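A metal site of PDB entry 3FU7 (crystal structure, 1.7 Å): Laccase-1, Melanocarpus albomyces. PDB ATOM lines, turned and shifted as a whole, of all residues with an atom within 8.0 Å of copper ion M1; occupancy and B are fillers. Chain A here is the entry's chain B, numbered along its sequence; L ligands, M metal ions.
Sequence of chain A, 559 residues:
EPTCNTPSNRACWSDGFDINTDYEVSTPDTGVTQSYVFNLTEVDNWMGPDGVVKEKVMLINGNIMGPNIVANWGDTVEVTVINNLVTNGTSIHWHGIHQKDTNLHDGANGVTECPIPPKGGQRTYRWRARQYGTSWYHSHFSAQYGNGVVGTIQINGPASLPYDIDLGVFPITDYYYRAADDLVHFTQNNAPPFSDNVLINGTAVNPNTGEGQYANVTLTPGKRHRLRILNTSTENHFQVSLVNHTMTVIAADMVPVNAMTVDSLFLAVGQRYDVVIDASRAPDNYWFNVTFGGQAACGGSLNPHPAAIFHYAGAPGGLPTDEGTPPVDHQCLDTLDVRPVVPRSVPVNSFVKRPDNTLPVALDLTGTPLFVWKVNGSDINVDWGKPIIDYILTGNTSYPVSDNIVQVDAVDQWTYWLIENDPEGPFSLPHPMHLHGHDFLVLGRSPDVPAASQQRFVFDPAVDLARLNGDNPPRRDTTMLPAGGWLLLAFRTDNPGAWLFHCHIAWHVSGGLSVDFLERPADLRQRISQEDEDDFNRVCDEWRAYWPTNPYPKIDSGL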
ATOM      1  N   HIS A  93     -28.347 -23.600   7.654  1.00  0.00           N
ATOM      2  CA  HIS A  93     -27.109 -24.082   7.113  1.00  0.00           C
ATOM      3  C   HIS A  93     -26.841 -25.500   7.606  1.00  0.00           C
ATOM      4  O   HIS A  93     -27.069 -25.808   8.779  1.00  0.00           O
ATOM      5  CB  HIS A  93     -25.954 -23.158   7.538  1.00  0.00           C
ATOM      6  CG  HIS A  93     -24.602 -23.703   7.225  1.00  0.00           C
ATOM      7  ND1 HIS A  93     -24.245 -24.084   5.950  1.00  0.00           N
ATOM      8  CD2 HIS A  93     -23.539 -23.963   8.017  1.00  0.00           C
ATOM      9  CE1 HIS A  93     -23.002 -24.531   5.972  1.00  0.00           C
ATOM     10  NE2 HIS A  93     -22.556 -24.472   7.204  1.00  0.00           N
ATOM     11  N   TRP A  94     -26.346 -26.359   6.716  1.00  0.00           N
ATOM     12  CA  TRP A  94     -26.169 -27.798   6.989  1.00  0.00           C
ATOM     13  C   TRP A  94     -24.679 -27.988   7.182  1.00  0.00           C
ATOM     14  O   TRP A  94     -23.916 -28.174   6.240  1.00  0.00           O
ATOM     15  CB  TRP A  94     -26.746 -28.614   5.800  1.00  0.00           C
ATOM     16  CG  TRP A  94     -28.074 -28.043   5.381  1.00  0.00           C
ATOM     17  CD1 TRP A  94     -28.289 -27.102   4.401  1.00  0.00           C
ATOM     18  CD2 TRP A  94     -29.367 -28.259   6.003  1.00  0.00           C
ATOM     19  NE1 TRP A  94     -29.618 -26.772   4.342  1.00  0.00           N
ATOM     20  CE2 TRP A  94     -30.305 -27.443   5.324  1.00  0.00           C
ATOM     21  CE3 TRP A  94     -29.823 -29.081   7.049  1.00  0.00           C
ATOM     22  CZ2 TRP A  94     -31.670 -27.425   5.647  1.00  0.00           C
ATOM     23  CZ3 TRP A  94     -31.179 -29.054   7.387  1.00  0.00           C
ATOM     24  CH2 TRP A  94     -32.092 -28.217   6.681  1.00  0.00           C
ATOM     25  N   HIS A  95     -24.279 -27.875   8.438  1.00  0.00           N
ATOM     26  CA  HIS A  95     -22.868 -27.743   8.782  1.00  0.00           C
ATOM     27  C   HIS A  95     -22.160 -29.072   8.605  1.00  0.00           C
ATOM     28  O   HIS A  95     -22.483 -30.048   9.294  1.00  0.00           O
ATOM     29  CB  HIS A  95     -22.748 -27.232  10.214  1.00  0.00           C
ATOM     30  CG  HIS A  95     -21.336 -27.105  10.678  1.00  0.00           C
ATOM     31  ND1 HIS A  95     -20.866 -25.987  11.315  1.00  0.00           N
ATOM     32  CD2 HIS A  95     -20.295 -27.975  10.634  1.00  0.00           C
ATOM     33  CE1 HIS A  95     -19.595 -26.153  11.629  1.00  0.00           C
ATOM     34  NE2 HIS A  95     -19.219 -27.359  11.218  1.00  0.00           N
ATOM     35  N   GLY A  96     -21.201 -29.118   7.684  1.00  0.00           N
ATOM     36  CA  GLY A  96     -20.492 -30.361   7.432  1.00  0.00           C
ATOM     37  C   GLY A  96     -20.958 -31.049   6.168  1.00  0.00           C
ATOM     38  O   GLY A  96     -20.357 -32.022   5.734  1.00  0.00           O
ATOM     39  N   TRP A 136     -24.539 -31.328  11.885  1.00  0.00           N
ATOM     40  CA  TRP A 136     -25.563 -30.524  12.555  1.00  0.00           C
ATOM     41  C   TRP A 136     -26.025 -29.425  11.633  1.00  0.00           C
ATOM     42  O   TRP A 136     -25.472 -29.241  10.542  1.00  0.00           O
ATOM     43  CB  TRP A 136     -25.068 -29.971  13.904  1.00  0.00           C
ATOM     44  CG  TRP A 136     -23.944 -28.978  13.903  1.00  0.00           C
ATOM     45  CD1 TRP A 136     -22.674 -29.134  13.418  1.00  0.00           C
ATOM     46  CD2 TRP A 136     -23.995 -27.694  14.503  1.00  0.00           C
ATOM     47  NE1 TRP A 136     -21.930 -27.985  13.663  1.00  0.00           N
ATOM     48  CE2 TRP A 136     -22.713 -27.086  14.327  1.00  0.00           C
ATOM     49  CE3 TRP A 136     -24.992 -26.989  15.173  1.00  0.00           C
ATOM     50  CZ2 TRP A 136     -22.413 -25.801  14.790  1.00  0.00           C
ATOM     51  CZ3 TRP A 136     -24.696 -25.698  15.649  1.00  0.00           C
ATOM     52  CH2 TRP A 136     -23.412 -25.119  15.463  1.00  0.00           C
ATOM     53  N   TYR A 137     -27.107 -28.756  12.011  1.00  0.00           N
ATOM     54  CA  TYR A 137     -27.613 -27.657  11.182  1.00  0.00           C
ATOM     55  C   TYR A 137     -28.014 -26.559  12.126  1.00  0.00           C
ATOM     56  O   TYR A 137     -28.327 -26.810  13.292  1.00  0.00           O
ATOM     57  CB  TYR A 137     -28.802 -28.105  10.311  1.00  0.00           C
ATOM     58  CG  TYR A 137     -29.994 -28.676  11.061  1.00  0.00           C
ATOM     59  CD1 TYR A 137     -30.953 -27.844  11.623  1.00  0.00           C
ATOM     60  CD2 TYR A 137     -30.140 -30.066  11.216  1.00  0.00           C
ATOM     61  CE1 TYR A 137     -32.029 -28.349  12.331  1.00  0.00           C
ATOM     62  CE2 TYR A 137     -31.228 -30.592  11.929  1.00  0.00           C
ATOM     63  CZ  TYR A 137     -32.164 -29.711  12.475  1.00  0.00           C
ATOM     64  OH  TYR A 137     -33.251 -30.187  13.173  1.00  0.00           O
ATOM     65  N   HIS A 138     -28.027 -25.329  11.625  1.00  0.00           N
ATOM     66  CA  HIS A 138     -28.350 -24.192  12.460  1.00  0.00           C
ATOM     67  C   HIS A 138     -28.703 -23.030  11.554  1.00  0.00           C
ATOM     68  O   HIS A 138     -28.231 -22.979  10.418  1.00  0.00           O
ATOM     69  CB  HIS A 138     -27.152 -23.810  13.377  1.00  0.00           C
ATOM     70  CG  HIS A 138     -25.851 -23.589  12.656  1.00  0.00           C
ATOM     71  ND1 HIS A 138     -25.548 -22.390  12.047  1.00  0.00           N
ATOM     72  CD2 HIS A 138     -24.769 -24.377  12.503  1.00  0.00           C
ATOM     73  CE1 HIS A 138     -24.330 -22.460  11.518  1.00  0.00           C
ATOM     74  NE2 HIS A 138     -23.848 -23.670  11.773  1.00  0.00           N
ATOM     75  N   SER A 139     -29.505 -22.087  12.048  1.00  0.00           N
ATOM     76  CA  SER A 139     -29.719 -20.795  11.348  1.00  0.00           C
ATOM     77  C   SER A 139     -28.390 -20.100  11.095  1.00  0.00           C
ATOM     78  O   SER A 139     -27.433 -20.227  11.876  1.00  0.00           O
ATOM     79  CB  SER A 139     -30.596 -19.865  12.195  1.00  0.00           C
ATOM     80  OG  SER A 139     -30.733 -18.607  11.571  1.00  0.00           O
ATOM     81  N   HIS A 140     -28.296 -19.377   9.999  1.00  0.00           N
ATOM     82  CA  HIS A 140     -27.116 -18.529   9.801  1.00  0.00           C
ATOM     83  C   HIS A 140     -27.520 -17.053   9.762  1.00  0.00           C
ATOM     84  O   HIS A 140     -26.752 -16.222   9.290  1.00  0.00           O
ATOM     85  CB  HIS A 140     -26.408 -18.887   8.496  1.00  0.00           C
ATOM     86  CG  HIS A 140     -24.927 -19.030   8.629  1.00  0.00           C
ATOM     87  ND1 HIS A 140     -24.146 -18.107   9.281  1.00  0.00           N
ATOM     88  CD2 HIS A 140     -24.095 -20.021   8.235  1.00  0.00           C
ATOM     89  CE1 HIS A 140     -22.886 -18.501   9.250  1.00  0.00           C
ATOM     90  NE2 HIS A 140     -22.829 -19.656   8.613  1.00  0.00           N
ATOM     91  N   TYR A 145     -29.205 -18.813  15.827  1.00  0.00           N
ATOM     92  CA  TYR A 145     -29.150 -20.215  16.296  1.00  0.00           C
ATOM     93  C   TYR A 145     -29.012 -20.326  17.812  1.00  0.00           C
ATOM     94  O   TYR A 145     -29.466 -21.309  18.402  1.00  0.00           O
ATOM     95  CB  TYR A 145     -28.147 -21.087  15.522  1.00  0.00           C
ATOM     96  CG  TYR A 145     -26.681 -21.113  15.923  1.00  0.00           C
ATOM     97  CD1 TYR A 145     -26.208 -22.050  16.850  1.00  0.00           C
ATOM     98  CD2 TYR A 145     -25.751 -20.300  15.285  1.00  0.00           C
ATOM     99  CE1 TYR A 145     -24.851 -22.120  17.185  1.00  0.00           C
ATOM    100  CE2 TYR A 145     -24.381 -20.368  15.599  1.00  0.00           C
ATOM    101  CZ  TYR A 145     -23.941 -21.296  16.527  1.00  0.00           C
ATOM    102  OH  TYR A 145     -22.606 -21.377  16.844  1.00  0.00           O
ATOM    103  N   ASN A 231     -20.406 -30.330  19.496  1.00  0.00           N
ATOM    104  CA  ASN A 231     -20.464 -29.059  20.223  1.00  0.00           C
ATOM    105  C   ASN A 231     -21.235 -28.047  19.396  1.00  0.00           C
ATOM    106  O   ASN A 231     -20.704 -27.498  18.422  1.00  0.00           O
ATOM    107  CB  ASN A 231     -19.055 -28.538  20.490  1.00  0.00           C
ATOM    108  CG  ASN A 231     -19.052 -27.201  21.247  1.00  0.00           C
ATOM    109  OD1 ASN A 231     -20.086 -26.597  21.516  1.00  0.00           O
ATOM    110  ND2 ASN A 231     -17.857 -26.729  21.580  1.00  0.00           N
ATOM    111  N   THR A 232     -22.513 -27.834  19.777  1.00  0.00           N
ATOM    112  CA  THR A 232     -23.409 -26.933  19.037  1.00  0.00           C
ATOM    113  C   THR A 232     -23.531 -25.551  19.662  1.00  0.00           C
ATOM    114  O   THR A 232     -24.538 -24.836  19.447  1.00  0.00           O
ATOM    115  CB  THR A 232     -24.801 -27.590  18.877  1.00  0.00           C
ATOM    116  OG1 THR A 232     -25.342 -27.864  20.182  1.00  0.00           O
ATOM    117  CG2 THR A 232     -24.674 -28.914  18.125  1.00  0.00           C
ATOM    118  N   SER A 233     -22.508 -25.160  20.406  1.00  0.00           N
ATOM    119  CA  SER A 233     -22.458 -23.897  21.124  1.00  0.00           C
ATOM    120  C   SER A 233     -22.405 -22.672  20.236  1.00  0.00           C
ATOM    121  O   SER A 233     -22.093 -22.776  19.064  1.00  0.00           O
ATOM    122  CB  SER A 233     -21.218 -23.859  22.004  1.00  0.00           C
ATOM    123  OG  SER A 233     -21.381 -24.721  23.104  1.00  0.00           O
ATOM    124  N   VAL A 269     -16.192 -25.146  19.000  1.00  0.00           N
ATOM    125  CA  VAL A 269     -17.555 -24.856  18.503  1.00  0.00           C
ATOM    126  C   VAL A 269     -17.684 -25.432  17.101  1.00  0.00           C
ATOM    127  O   VAL A 269     -16.870 -25.141  16.219  1.00  0.00           O
ATOM    128  CB  VAL A 269     -17.761 -23.354  18.420  1.00  0.00           C
ATOM    129  CG1 VAL A 269     -19.114 -23.030  17.727  1.00  0.00           C
ATOM    130  CG2 VAL A 269     -17.692 -22.765  19.812  1.00  0.00           C
ATOM    131  N   GLY A 270     -18.721 -26.225  16.908  1.00  0.00           N
ATOM    132  CA  GLY A 270     -18.997 -26.789  15.614  1.00  0.00           C
ATOM    133  C   GLY A 270     -18.313 -28.103  15.338  1.00  0.00           C
ATOM    134  O   GLY A 270     -18.636 -28.761  14.348  1.00  0.00           O
ATOM    135  N   GLN A 271     -17.386 -28.514  16.209  1.00  0.00           N
ATOM    136  CA  GLN A 271     -16.742 -29.815  16.028  1.00  0.00           C
ATOM    137  C   GLN A 271     -17.583 -31.009  16.466  1.00  0.00           C
ATOM    138  O   GLN A 271     -18.486 -30.895  17.313  1.00  0.00           O
ATOM    139  CB  GLN A 271     -15.341 -29.895  16.682  1.00  0.00           C
ATOM    140  CG  GLN A 271     -14.267 -29.155  15.906  1.00  0.00           C
ATOM    141  CD  GLN A 271     -12.891 -29.345  16.482  1.00  0.00           C
ATOM    142  OE1 GLN A 271     -12.733 -29.549  17.688  1.00  0.00           O
ATOM    143  NE2 GLN A 271     -11.878 -29.254  15.620  1.00  0.00           N
ATOM    144  N   ARG A 272     -17.288 -32.149  15.845  1.00  0.00           N
ATOM    145  CA  ARG A 272     -17.908 -33.440  16.217  1.00  0.00           C
ATOM    146  C   ARG A 272     -16.869 -34.520  16.335  1.00  0.00           C
ATOM    147  O   ARG A 272     -15.843 -34.499  15.661  1.00  0.00           O
ATOM    148  CB  ARG A 272     -18.964 -33.915  15.189  1.00  0.00           C
ATOM    149  CG  ARG A 272     -20.208 -33.069  15.109  1.00  0.00           C
ATOM    150  CD  ARG A 272     -20.005 -31.921  14.095  1.00  0.00           C
ATOM    151  NE  ARG A 272     -19.878 -32.389  12.710  1.00  0.00           N
ATOM    152  CZ  ARG A 272     -19.258 -31.711  11.751  1.00  0.00           C
ATOM    153  NH1 ARG A 272     -18.640 -30.551  12.015  1.00  0.00           N
ATOM    154  NH2 ARG A 272     -19.193 -32.213  10.527  1.00  0.00           N
ATOM    155  N   HIS A 434     -13.988 -22.419  10.557  1.00  0.00           N
ATOM    156  CA  HIS A 434     -14.842 -23.371   9.862  1.00  0.00           C
ATOM    157  C   HIS A 434     -15.014 -22.994   8.384  1.00  0.00           C
ATOM    158  O   HIS A 434     -15.268 -21.827   8.079  1.00  0.00           O
ATOM    159  CB  HIS A 434     -16.208 -23.404  10.541  1.00  0.00           C
ATOM    160  CG  HIS A 434     -17.240 -24.129   9.745  1.00  0.00           C
ATOM    161  ND1 HIS A 434     -17.068 -25.443   9.351  1.00  0.00           N
ATOM    162  CD2 HIS A 434     -18.433 -23.732   9.253  1.00  0.00           C
ATOM    163  CE1 HIS A 434     -18.125 -25.825   8.649  1.00  0.00           C
ATOM    164  NE2 HIS A 434     -18.970 -24.807   8.579  1.00  0.00           N
ATOM    165  N   HIS A 436     -17.024 -23.719   4.797  1.00  0.00           N
ATOM    166  CA  HIS A 436     -18.185 -24.273   4.087  1.00  0.00           C
ATOM    167  C   HIS A 436     -17.718 -24.936   2.776  1.00  0.00           C
ATOM    168  O   HIS A 436     -16.670 -24.559   2.237  1.00  0.00           O
ATOM    169  CB  HIS A 436     -19.155 -23.156   3.685  1.00  0.00           C
ATOM    170  CG  HIS A 436     -19.925 -22.542   4.817  1.00  0.00           C
ATOM    171  ND1 HIS A 436     -21.251 -22.173   4.681  1.00  0.00           N
ATOM    172  CD2 HIS A 436     -19.561 -22.176   6.066  1.00  0.00           C
ATOM    173  CE1 HIS A 436     -21.660 -21.623   5.812  1.00  0.00           C
ATOM    174  NE2 HIS A 436     -20.665 -21.628   6.669  1.00  0.00           N
ATOM    175  N   ASP A 477     -13.763 -30.091   8.975  1.00  0.00           N
ATOM    176  CA  ASP A 477     -14.371 -28.817   8.603  1.00  0.00           C
ATOM    177  C   ASP A 477     -14.186 -27.663   9.588  1.00  0.00           C
ATOM    178  O   ASP A 477     -14.437 -26.504   9.246  1.00  0.00           O
ATOM    179  CB  ASP A 477     -15.868 -28.972   8.206  1.00  0.00           C
ATOM    180  CG  ASP A 477     -16.758 -29.355   9.356  1.00  0.00           C
ATOM    181  OD1 ASP A 477     -16.806 -28.605  10.362  1.00  0.00           O
ATOM    182  OD2 ASP A 477     -17.465 -30.392   9.232  1.00  0.00           O
ATOM    183  N   THR A 478     -13.709 -27.970  10.789  1.00  0.00           N
ATOM    184  CA  THR A 478     -13.469 -26.967  11.802  1.00  0.00           C
ATOM    185  C   THR A 478     -12.179 -27.317  12.560  1.00  0.00           C
ATOM    186  O   THR A 478     -11.998 -28.483  12.922  1.00  0.00           O
ATOM    187  CB  THR A 478     -14.634 -26.963  12.780  1.00  0.00           C
ATOM    188  OG1 THR A 478     -15.868 -26.675  12.088  1.00  0.00           O
ATOM    189  CG2 THR A 478     -14.403 -25.891  13.862  1.00  0.00           C
ATOM    190  N   HIS A 502     -14.999 -18.865   8.292  1.00  0.00           N
ATOM    191  CA  HIS A 502     -15.268 -17.930   9.379  1.00  0.00           C
ATOM    192  C   HIS A 502     -15.014 -18.541  10.745  1.00  0.00           C
ATOM    193  O   HIS A 502     -15.033 -19.759  10.907  1.00  0.00           O
ATOM    194  CB  HIS A 502     -16.707 -17.396   9.295  1.00  0.00           C
ATOM    195  CG  HIS A 502     -17.792 -18.406   9.516  1.00  0.00           C
ATOM    196  ND1 HIS A 502     -18.267 -18.734  10.773  1.00  0.00           N
ATOM    197  CD2 HIS A 502     -18.505 -19.138   8.635  1.00  0.00           C
ATOM    198  CE1 HIS A 502     -19.237 -19.637  10.641  1.00  0.00           C
ATOM    199  NE2 HIS A 502     -19.392 -19.910   9.367  1.00  0.00           N
ATOM    200  N   HIS A 504     -16.339 -19.665  14.171  1.00  0.00           N
ATOM    201  CA  HIS A 504     -17.708 -20.089  14.515  1.00  0.00           C
ATOM    202  C   HIS A 504     -18.148 -19.562  15.887  1.00  0.00           C
ATOM    203  O   HIS A 504     -19.238 -19.922  16.377  1.00  0.00           O
ATOM    204  CB  HIS A 504     -17.808 -21.614  14.471  1.00  0.00           C
ATOM    205  CG  HIS A 504     -19.122 -22.111  13.978  1.00  0.00           C
ATOM    206  ND1 HIS A 504     -20.293 -21.966  14.709  1.00  0.00           N
ATOM    207  CD2 HIS A 504     -19.458 -22.755  12.844  1.00  0.00           C
ATOM    208  CE1 HIS A 504     -21.293 -22.497  14.018  1.00  0.00           C
ATOM    209  NE2 HIS A 504     -20.802 -22.982  12.891  1.00  0.00           N
HETATM  210  O1  LIG L   1     -21.659 -21.977  10.402  1.00  0.00           O
HETATM  211  O2  LIG L   1     -21.202 -22.628   9.677  1.00  0.00           O
HETATM  212 CU    CU M   1     -21.920 -24.289  11.687  1.00  0.00          CU
HETATM  213 CU    CU M   2     -20.764 -24.742   7.847  1.00  0.00          CU
HETATM  214 CU    CU M   3     -20.999 -20.693   8.395  1.00  0.00          CU
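A ring nitrogen (NE2) of His 95 lies within hydrogen-bond range of the side-chain carboxylate of Asp 477.
The backbone carbonyl oxygen (O) of Gly 270 sits at hydrogen-bond distance from a ring nitrogen (NE2) of His 95, 3.5 Å away.
A ring nitrogen (NE2) of His 95 is in hydrogen-bond range of the guanidinium group (NH1) of Arg 272, at 3.3 Å.
NE1 of Trp 136 sits at hydrogen-bond distance from O of Gly 270 (3.5 Å).
NE2 of His 95 sits close to ND1 of His 434.
The backbone NH (N) of His 95 is in hydrogen-bond range of the backbone carbonyl oxygen (O) of Trp 136.
The backbone NH (N) of His 93 sits at hydrogen-bond distance from the backbone carbonyl oxygen (O) of His 138.
A ring nitrogen (ND1) of His 504 is in hydrogen-bond range of the side-chain hydroxyl (OH) of Tyr 145, at 3.2 Å.
Trp 136 touches copper ion M1 (CZ2 to CU, 3.5 Å).
NE2 of His 138 is bound to copper ion M1, at 2.0 Å.
ND1 of His 95 binds copper ion M1 (2.0 Å).
NE2 of His 504 is bound to copper ion M1 (2.1 Å).
Copper ion M1 has three donor atoms within binding distance.
Slightly farther from copper ion M1 lies O1 of the ligand (2.7 Å).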
